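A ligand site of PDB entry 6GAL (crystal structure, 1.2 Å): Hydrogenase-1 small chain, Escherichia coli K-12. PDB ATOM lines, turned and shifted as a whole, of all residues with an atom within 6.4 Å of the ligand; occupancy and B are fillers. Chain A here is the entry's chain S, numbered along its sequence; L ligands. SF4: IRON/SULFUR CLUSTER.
Residues that only touch the ligand: Arg 192 (3.7 Å), Ile 243 (3.7 Å), Tyr 217 (3.8 Å), Gly 223 (3.8 Å), Phe 196 (3.8 Å), Pro 224 (3.9 Å) and Ile 186 (3.99 Å).
Of the 25 residues printed, 13 come within 4 Å of the ligand.
The nearest printed residue that does not touch the ligand is Tyr 214 (5.4 Å).
The guanidinium group (NH2) of Arg 192 is in hydrogen-bond range of the side-chain hydroxyl (OH) of Tyr 191 (3.1 Å).
The guanidinium group of Arg 192 sits at hydrogen-bond distance from the backbone carbonyl oxygen of Tyr 214 (2.9 Å).
The backbone NH (N) of Arg 192 lies close to the side-chain sulfur (SG) of Cys 190.
O of Leu 216 lies within hydrogen-bond range of N of Cys 221.
The backbone NH of Gly 223 sits close to the side-chain sulfur of Cys 221 (3.3 Å).
The side-chain sulfur of Cys 215 lies close to the backbone NH of Tyr 217 (3.3 Å).
The backbone NH (N) of Cys 249 sits close to the side-chain sulfur (SG) of Cys 221 (3.4 Å).
O of Ile 243 sits at hydrogen-bond distance from NH2 of Arg 192.
The side-chain sulfur of Cys 190 is bound to an iron atom (FE4) of the ligand, at 2.3 Å.
The backbone NH (N) of Arg 193 sits close to a sulfur (S2) of the ligand (3.7 Å).
N of Leu 216 lies close to S3 of the ligand, 3.4 Å away.
The side-chain sulfur (SG) of Cys 221 is bound to an iron atom (FE2) of the ligand.
An iron atom (FE1) of the ligand is bound by the side-chain sulfur (SG) of Cys 215, at 2.3 Å.
ND1 of His 187 binds FE3 of the ligand.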
ATOM      1  N   ILE A 186      -4.448 -32.446 -29.386  1.00  0.00           N
ATOM      2  CA  ILE A 186      -5.558 -32.784 -28.512  1.00  0.00           C
ATOM      3  C   ILE A 186      -6.862 -32.153 -29.030  1.00  0.00           C
ATOM      4  O   ILE A 186      -7.888 -32.835 -29.136  1.00  0.00           O
ATOM      5  CB  ILE A 186      -5.278 -32.296 -27.053  1.00  0.00           C
ATOM      6  CG1 ILE A 186      -4.078 -33.020 -26.411  1.00  0.00           C
ATOM      7  CG2 ILE A 186      -6.503 -32.362 -26.185  1.00  0.00           C
ATOM      8  CD1 ILE A 186      -4.332 -34.496 -26.273  1.00  0.00           C
ATOM      9  N   HIS A 187      -6.786 -30.873 -29.359  1.00  0.00           N
ATOM     10  CA  HIS A 187      -7.957 -30.039 -29.805  1.00  0.00           C
ATOM     11  C   HIS A 187      -8.464 -30.461 -31.203  1.00  0.00           C
ATOM     12  O   HIS A 187      -9.566 -30.050 -31.585  1.00  0.00           O
ATOM     13  CB  HIS A 187      -7.462 -28.593 -29.765  1.00  0.00           C
ATOM     14  CG  HIS A 187      -8.394 -27.504 -30.193  1.00  0.00           C
ATOM     15  ND1 HIS A 187      -9.397 -26.986 -29.374  1.00  0.00           N
ATOM     16  CD2 HIS A 187      -8.321 -26.677 -31.265  1.00  0.00           C
ATOM     17  CE1 HIS A 187      -9.922 -25.922 -29.986  1.00  0.00           C
ATOM     18  NE2 HIS A 187      -9.294 -25.738 -31.136  1.00  0.00           N
ATOM     19  N   ASP A 188      -7.677 -31.214 -31.949  1.00  0.00           N
ATOM     20  CA  ASP A 188      -8.096 -31.756 -33.260  1.00  0.00           C
ATOM     21  C   ASP A 188      -9.018 -32.972 -33.113  1.00  0.00           C
ATOM     22  O   ASP A 188      -9.602 -33.416 -34.112  1.00  0.00           O
ATOM     23  CB  ASP A 188      -6.901 -32.175 -34.120  1.00  0.00           C
ATOM     24  CG  ASP A 188      -5.950 -31.024 -34.488  1.00  0.00           C
ATOM     25  OD1 ASP A 188      -6.387 -29.874 -34.580  1.00  0.00           O
ATOM     26  OD2 ASP A 188      -4.722 -31.309 -34.718  1.00  0.00           O
ATOM     27  N   CYS A 190     -10.891 -33.404 -29.869  1.00  0.00           N
ATOM     28  CA  CYS A 190     -11.528 -33.203 -28.574  1.00  0.00           C
ATOM     29  C   CYS A 190     -13.044 -33.225 -28.702  1.00  0.00           C
ATOM     30  O   CYS A 190     -13.642 -32.492 -29.517  1.00  0.00           O
ATOM     31  CB  CYS A 190     -11.070 -31.900 -27.925  1.00  0.00           C
ATOM     32  SG  CYS A 190     -11.807 -31.655 -26.272  1.00  0.00           S
ATOM     33  N   TYR A 191     -13.677 -34.044 -27.855  1.00  0.00           N
ATOM     34  CA  TYR A 191     -15.139 -34.156 -27.826  1.00  0.00           C
ATOM     35  C   TYR A 191     -15.880 -32.915 -27.370  1.00  0.00           C
ATOM     36  O   TYR A 191     -17.122 -32.831 -27.491  1.00  0.00           O
ATOM     37  CB  TYR A 191     -15.590 -35.396 -27.040  1.00  0.00           C
ATOM     38  CG  TYR A 191     -15.685 -35.248 -25.556  1.00  0.00           C
ATOM     39  CD1 TYR A 191     -14.661 -34.696 -24.805  1.00  0.00           C
ATOM     40  CD2 TYR A 191     -16.830 -35.623 -24.910  1.00  0.00           C
ATOM     41  CE1 TYR A 191     -14.781 -34.535 -23.439  1.00  0.00           C
ATOM     42  CE2 TYR A 191     -16.972 -35.443 -23.544  1.00  0.00           C
ATOM     43  CZ  TYR A 191     -15.959 -34.886 -22.802  1.00  0.00           C
ATOM     44  OH  TYR A 191     -16.095 -34.694 -21.435  1.00  0.00           O
ATOM     45  N   ARG A 192     -15.151 -31.879 -26.872  1.00  0.00           N
ATOM     46  CA  ARG A 192     -15.788 -30.607 -26.530  1.00  0.00           C
ATOM     47  C   ARG A 192     -15.668 -29.560 -27.659  1.00  0.00           C
ATOM     48  O   ARG A 192     -16.095 -28.424 -27.458  1.00  0.00           O
ATOM     49  CB  ARG A 192     -15.287 -30.065 -25.207  1.00  0.00           C
ATOM     50  CG  ARG A 192     -15.533 -31.037 -24.061  1.00  0.00           C
ATOM     51  CD  ARG A 192     -15.258 -30.460 -22.692  1.00  0.00           C
ATOM     52  NE  ARG A 192     -15.503 -31.471 -21.663  1.00  0.00           N
ATOM     53  CZ  ARG A 192     -15.697 -31.243 -20.382  1.00  0.00           C
ATOM     54  NH1 ARG A 192     -15.709 -30.000 -19.901  1.00  0.00           N
ATOM     55  NH2 ARG A 192     -15.886 -32.270 -19.557  1.00  0.00           N
ATOM     56  N   ARG A 193     -15.175 -29.953 -28.825  1.00  0.00           N
ATOM     57  CA  ARG A 193     -15.013 -28.988 -29.930  1.00  0.00           C
ATOM     58  C   ARG A 193     -16.336 -28.379 -30.375  1.00  0.00           C
ATOM     59  O   ARG A 193     -16.370 -27.212 -30.764  1.00  0.00           O
ATOM     60  CB  ARG A 193     -14.288 -29.614 -31.106  1.00  0.00           C
ATOM     61  CG  ARG A 193     -12.792 -29.550 -31.023  1.00  0.00           C
ATOM     62  CD  ARG A 193     -12.270 -28.099 -31.137  1.00  0.00           C
ATOM     63  NE  ARG A 193     -12.490 -27.415 -32.405  1.00  0.00           N
ATOM     64  CZ  ARG A 193     -11.607 -27.304 -33.404  1.00  0.00           C
ATOM     65  NH1 ARG A 193     -10.448 -27.934 -33.390  1.00  0.00           N
ATOM     66  NH2 ARG A 193     -11.943 -26.583 -34.472  1.00  0.00           N
ATOM     67  N   ALA A 194     -17.428 -29.133 -30.267  1.00  0.00           N
ATOM     68  CA  ALA A 194     -18.730 -28.520 -30.603  1.00  0.00           C
ATOM     69  C   ALA A 194     -18.962 -27.239 -29.793  1.00  0.00           C
ATOM     70  O   ALA A 194     -19.495 -26.250 -30.304  1.00  0.00           O
ATOM     71  CB  ALA A 194     -19.855 -29.463 -30.319  1.00  0.00           C
ATOM     72  N   HIS A 195     -18.597 -27.312 -28.514  1.00  0.00           N
ATOM     73  CA  HIS A 195     -18.789 -26.160 -27.637  1.00  0.00           C
ATOM     74  C   HIS A 195     -17.800 -25.058 -27.982  1.00  0.00           C
ATOM     75  O   HIS A 195     -18.174 -23.891 -28.003  1.00  0.00           O
ATOM     76  CB  HIS A 195     -18.655 -26.611 -26.177  1.00  0.00           C
ATOM     77  CG  HIS A 195     -19.671 -27.653 -25.796  1.00  0.00           C
ATOM     78  ND1 HIS A 195     -21.042 -27.446 -25.918  1.00  0.00           N
ATOM     79  CD2 HIS A 195     -19.531 -28.902 -25.278  1.00  0.00           C
ATOM     80  CE1 HIS A 195     -21.677 -28.543 -25.505  1.00  0.00           C
ATOM     81  NE2 HIS A 195     -20.788 -29.424 -25.081  1.00  0.00           N
ATOM     82  N   PHE A 196     -16.542 -25.412 -28.202  1.00  0.00           N
ATOM     83  CA  PHE A 196     -15.564 -24.414 -28.651  1.00  0.00           C
ATOM     84  C   PHE A 196     -16.100 -23.637 -29.860  1.00  0.00           C
ATOM     85  O   PHE A 196     -16.073 -22.392 -29.869  1.00  0.00           O
ATOM     86  CB  PHE A 196     -14.229 -25.099 -28.983  1.00  0.00           C
ATOM     87  CG  PHE A 196     -13.185 -24.187 -29.467  1.00  0.00           C
ATOM     88  CD1 PHE A 196     -12.348 -23.517 -28.574  1.00  0.00           C
ATOM     89  CD2 PHE A 196     -12.966 -23.988 -30.844  1.00  0.00           C
ATOM     90  CE1 PHE A 196     -11.328 -22.687 -29.008  1.00  0.00           C
ATOM     91  CE2 PHE A 196     -11.956 -23.122 -31.272  1.00  0.00           C
ATOM     92  CZ  PHE A 196     -11.161 -22.480 -30.350  1.00  0.00           C
ATOM     93  N   PHE A 201     -18.441 -21.934 -23.268  1.00  0.00           N
ATOM     94  CA  PHE A 201     -17.289 -22.138 -22.429  1.00  0.00           C
ATOM     95  C   PHE A 201     -17.648 -22.186 -20.953  1.00  0.00           C
ATOM     96  O   PHE A 201     -18.477 -21.403 -20.438  1.00  0.00           O
ATOM     97  CB  PHE A 201     -16.356 -20.949 -22.611  1.00  0.00           C
ATOM     98  CG  PHE A 201     -15.878 -20.762 -24.003  1.00  0.00           C
ATOM     99  CD1 PHE A 201     -15.042 -21.703 -24.601  1.00  0.00           C
ATOM    100  CD2 PHE A 201     -16.229 -19.647 -24.734  1.00  0.00           C
ATOM    101  CE1 PHE A 201     -14.596 -21.526 -25.868  1.00  0.00           C
ATOM    102  CE2 PHE A 201     -15.773 -19.482 -26.029  1.00  0.00           C
ATOM    103  CZ  PHE A 201     -14.959 -20.397 -26.614  1.00  0.00           C
ATOM    104  N   TYR A 214     -19.042 -28.083 -21.092  1.00  0.00           N
ATOM    105  CA  TYR A 214     -18.608 -27.106 -22.063  1.00  0.00           C
ATOM    106  C   TYR A 214     -17.081 -27.025 -22.175  1.00  0.00           C
ATOM    107  O   TYR A 214     -16.332 -27.578 -21.384  1.00  0.00           O
ATOM    108  CB  TYR A 214     -19.222 -25.736 -21.739  1.00  0.00           C
ATOM    109  CG  TYR A 214     -20.693 -25.543 -22.150  1.00  0.00           C
ATOM    110  CD1 TYR A 214     -21.487 -26.596 -22.547  1.00  0.00           C
ATOM    111  CD2 TYR A 214     -21.268 -24.290 -22.018  1.00  0.00           C
ATOM    112  CE1 TYR A 214     -22.840 -26.404 -22.875  1.00  0.00           C
ATOM    113  CE2 TYR A 214     -22.601 -24.068 -22.342  1.00  0.00           C
ATOM    114  CZ  TYR A 214     -23.371 -25.133 -22.769  1.00  0.00           C
ATOM    115  OH  TYR A 214     -24.677 -24.963 -23.092  1.00  0.00           O
ATOM    116  N   CYS A 215     -16.635 -26.342 -23.228  1.00  0.00           N
ATOM    117  CA  CYS A 215     -15.232 -26.208 -23.539  1.00  0.00           C
ATOM    118  C   CYS A 215     -14.476 -25.464 -22.432  1.00  0.00           C
ATOM    119  O   CYS A 215     -15.012 -24.546 -21.798  1.00  0.00           O
ATOM    120  CB  CYS A 215     -15.054 -25.553 -24.930  1.00  0.00           C
ATOM    121  SG  CYS A 215     -13.371 -25.026 -25.347  1.00  0.00           S
ATOM    122  N   LEU A 216     -13.216 -25.892 -22.251  1.00  0.00           N
ATOM    123  CA  LEU A 216     -12.332 -25.402 -21.174  1.00  0.00           C
ATOM    124  C   LEU A 216     -11.312 -24.376 -21.653  1.00  0.00           C
ATOM    125  O   LEU A 216     -10.416 -24.007 -20.870  1.00  0.00           O
ATOM    126  CB  LEU A 216     -11.660 -26.605 -20.514  1.00  0.00           C
ATOM    127  CG  LEU A 216     -12.619 -27.575 -19.847  1.00  0.00           C
ATOM    128  CD1 LEU A 216     -11.945 -28.847 -19.426  1.00  0.00           C
ATOM    129  CD2 LEU A 216     -13.381 -26.978 -18.690  1.00  0.00           C
ATOM    130  N   TYR A 217     -11.468 -23.855 -22.863  1.00  0.00           N
ATOM    131  CA  TYR A 217     -10.545 -22.831 -23.392  1.00  0.00           C
ATOM    132  C   TYR A 217     -10.365 -21.650 -22.455  1.00  0.00           C
ATOM    133  O   TYR A 217      -9.214 -21.177 -22.225  1.00  0.00           O
ATOM    134  CB  TYR A 217     -11.067 -22.394 -24.772  1.00  0.00           C
ATOM    135  CG  TYR A 217     -10.375 -21.136 -25.292  1.00  0.00           C
ATOM    136  CD1 TYR A 217      -9.093 -21.147 -25.766  1.00  0.00           C
ATOM    137  CD2 TYR A 217     -11.083 -19.930 -25.263  1.00  0.00           C
ATOM    138  CE1 TYR A 217      -8.465 -19.954 -26.167  1.00  0.00           C
ATOM    139  CE2 TYR A 217     -10.490 -18.759 -25.671  1.00  0.00           C
ATOM    140  CZ  TYR A 217      -9.193 -18.786 -26.113  1.00  0.00           C
ATOM    141  OH  TYR A 217      -8.614 -17.601 -26.511  1.00  0.00           O
ATOM    142  N   LYS A 218     -11.461 -21.094 -21.938  1.00  0.00           N
ATOM    143  CA  LYS A 218     -11.360 -19.899 -21.095  1.00  0.00           C
ATOM    144  C   LYS A 218     -10.811 -20.192 -19.694  1.00  0.00           C
ATOM    145  O   LYS A 218     -10.439 -19.288 -18.981  1.00  0.00           O
ATOM    146  CB  LYS A 218     -12.693 -19.143 -20.976  1.00  0.00           C
ATOM    147  CG  LYS A 218     -13.134 -18.580 -22.323  1.00  0.00           C
ATOM    148  CD  LYS A 218     -14.325 -17.656 -22.204  1.00  0.00           C
ATOM    149  CE  LYS A 218     -14.530 -16.846 -23.480  1.00  0.00           C
ATOM    150  NZ  LYS A 218     -15.739 -16.015 -23.355  1.00  0.00           N
ATOM    151  N   CYS A 221      -7.252 -24.231 -21.063  1.00  0.00           N
ATOM    152  CA  CYS A 221      -6.888 -25.450 -21.764  1.00  0.00           C
ATOM    153  C   CYS A 221      -5.828 -25.226 -22.835  1.00  0.00           C
ATOM    154  O   CYS A 221      -6.034 -24.348 -23.724  1.00  0.00           O
ATOM    155  CB  CYS A 221      -8.125 -26.012 -22.430  1.00  0.00           C
ATOM    156  SG  CYS A 221      -7.870 -27.600 -23.242  1.00  0.00           S
ATOM    157  N   LYS A 222      -4.794 -26.039 -22.815  1.00  0.00           N
ATOM    158  CA  LYS A 222      -3.715 -25.935 -23.814  1.00  0.00           C
ATOM    159  C   LYS A 222      -3.852 -26.962 -24.934  1.00  0.00           C
ATOM    160  O   LYS A 222      -2.921 -27.180 -25.747  1.00  0.00           O
ATOM    161  CB  LYS A 222      -2.349 -26.019 -23.114  1.00  0.00           C
ATOM    162  CG  LYS A 222      -2.154 -24.893 -22.091  1.00  0.00           C
ATOM    163  CD  LYS A 222      -2.460 -23.526 -22.692  1.00  0.00           C
ATOM    164  CE  LYS A 222      -2.215 -22.328 -21.855  1.00  0.00           C
ATOM    165  NZ  LYS A 222      -2.634 -22.410 -20.441  1.00  0.00           N
ATOM    166  N   GLY A 223      -5.026 -27.606 -24.999  1.00  0.00           N
ATOM    167  CA  GLY A 223      -5.256 -28.543 -26.066  1.00  0.00           C
ATOM    168  C   GLY A 223      -4.974 -28.014 -27.475  1.00  0.00           C
ATOM    169  O   GLY A 223      -4.461 -28.747 -28.315  1.00  0.00           O
ATOM    170  N   PRO A 224      -5.269 -26.710 -27.723  1.00  0.00           N
ATOM    171  CA  PRO A 224      -4.994 -26.194 -29.066  1.00  0.00           C
ATOM    172  C   PRO A 224      -3.554 -26.186 -29.541  1.00  0.00           C
ATOM    173  O   PRO A 224      -3.342 -26.064 -30.736  1.00  0.00           O
ATOM    174  CB  PRO A 224      -5.561 -24.750 -29.011  1.00  0.00           C
ATOM    175  CG  PRO A 224      -6.708 -24.885 -28.042  1.00  0.00           C
ATOM    176  CD  PRO A 224      -6.169 -25.795 -26.954  1.00  0.00           C
ATOM    177  N   PHE A 241      -9.777 -38.601 -19.705  1.00  0.00           N
ATOM    178  CA  PHE A 241      -8.570 -37.813 -19.946  1.00  0.00           C
ATOM    179  C   PHE A 241      -8.778 -36.496 -19.250  1.00  0.00           C
ATOM    180  O   PHE A 241      -9.888 -36.222 -18.761  1.00  0.00           O
ATOM    181  CB  PHE A 241      -8.208 -37.735 -21.432  1.00  0.00           C
ATOM    182  CG  PHE A 241      -9.027 -36.758 -22.287  1.00  0.00           C
ATOM    183  CD1 PHE A 241     -10.335 -37.032 -22.623  1.00  0.00           C
ATOM    184  CD2 PHE A 241      -8.410 -35.636 -22.884  1.00  0.00           C
ATOM    185  CE1 PHE A 241     -11.065 -36.191 -23.464  1.00  0.00           C
ATOM    186  CE2 PHE A 241      -9.112 -34.823 -23.746  1.00  0.00           C
ATOM    187  CZ  PHE A 241     -10.434 -35.076 -24.034  1.00  0.00           C
ATOM    188  N   ILE A 243      -9.434 -33.324 -19.874  1.00  0.00           N
ATOM    189  CA  ILE A 243     -10.550 -32.478 -20.253  1.00  0.00           C
ATOM    190  C   ILE A 243     -11.867 -33.167 -19.937  1.00  0.00           C
ATOM    191  O   ILE A 243     -12.800 -32.515 -19.498  1.00  0.00           O
ATOM    192  CB  ILE A 243     -10.435 -32.104 -21.739  1.00  0.00           C
ATOM    193  CG1 ILE A 243      -9.315 -31.081 -21.936  1.00  0.00           C
ATOM    194  CG2 ILE A 243     -11.764 -31.671 -22.337  1.00  0.00           C
ATOM    195  CD1 ILE A 243      -8.615 -31.226 -23.256  1.00  0.00           C
ATOM    196  N   GLY A 248      -8.645 -28.283 -17.972  1.00  0.00           N
ATOM    197  CA  GLY A 248      -8.022 -28.103 -19.259  1.00  0.00           C
ATOM    198  C   GLY A 248      -6.723 -28.844 -19.358  1.00  0.00           C
ATOM    199  O   GLY A 248      -6.048 -29.107 -18.360  1.00  0.00           O
ATOM    200  N   CYS A 249      -6.355 -29.193 -20.588  1.00  0.00           N
ATOM    201  CA  CYS A 249      -4.997 -29.694 -20.822  1.00  0.00           C
ATOM    202  C   CYS A 249      -3.984 -28.651 -20.312  1.00  0.00           C
ATOM    203  O   CYS A 249      -4.136 -27.462 -20.484  1.00  0.00           O
ATOM    204  CB  CYS A 249      -4.870 -29.944 -22.335  1.00  0.00           C
ATOM    205  SG  CYS A 249      -3.260 -30.412 -22.992  1.00  0.00           S
ATOM    206  N   VAL A 267      -4.664 -19.888 -24.049  1.00  0.00           N
ATOM    207  CA  VAL A 267      -3.642 -20.203 -25.034  1.00  0.00           C
ATOM    208  C   VAL A 267      -3.508 -19.069 -26.049  1.00  0.00           C
ATOM    209  O   VAL A 267      -4.488 -18.311 -26.301  1.00  0.00           O
ATOM    210  CB  VAL A 267      -3.958 -21.619 -25.647  1.00  0.00           C
ATOM    211  CG1 VAL A 267      -5.221 -21.566 -26.467  1.00  0.00           C
ATOM    212  CG2 VAL A 267      -2.794 -22.134 -26.459  1.00  0.00           C
HETATM  213 FE1  SF4 L   1     -11.999 -26.814 -25.710  1.00  0.00          FE
HETATM  214 FE2  SF4 L   1      -9.556 -27.725 -24.816  1.00  0.00          FE
HETATM  215 FE3  SF4 L   1     -10.052 -27.500 -27.470  1.00  0.00          FE
HETATM  216 FE4  SF4 L   1     -11.251 -29.434 -26.055  1.00  0.00          FE
HETATM  217  S1  SF4 L   1      -8.971 -29.234 -26.473  1.00  0.00           S
HETATM  218  S2  SF4 L   1     -12.286 -28.092 -27.591  1.00  0.00           S
HETATM  219  S3  SF4 L   1     -11.666 -28.360 -24.048  1.00  0.00           S
HETATM  220  S4  SF4 L   1      -9.928 -25.776 -25.964  1.00  0.00           S
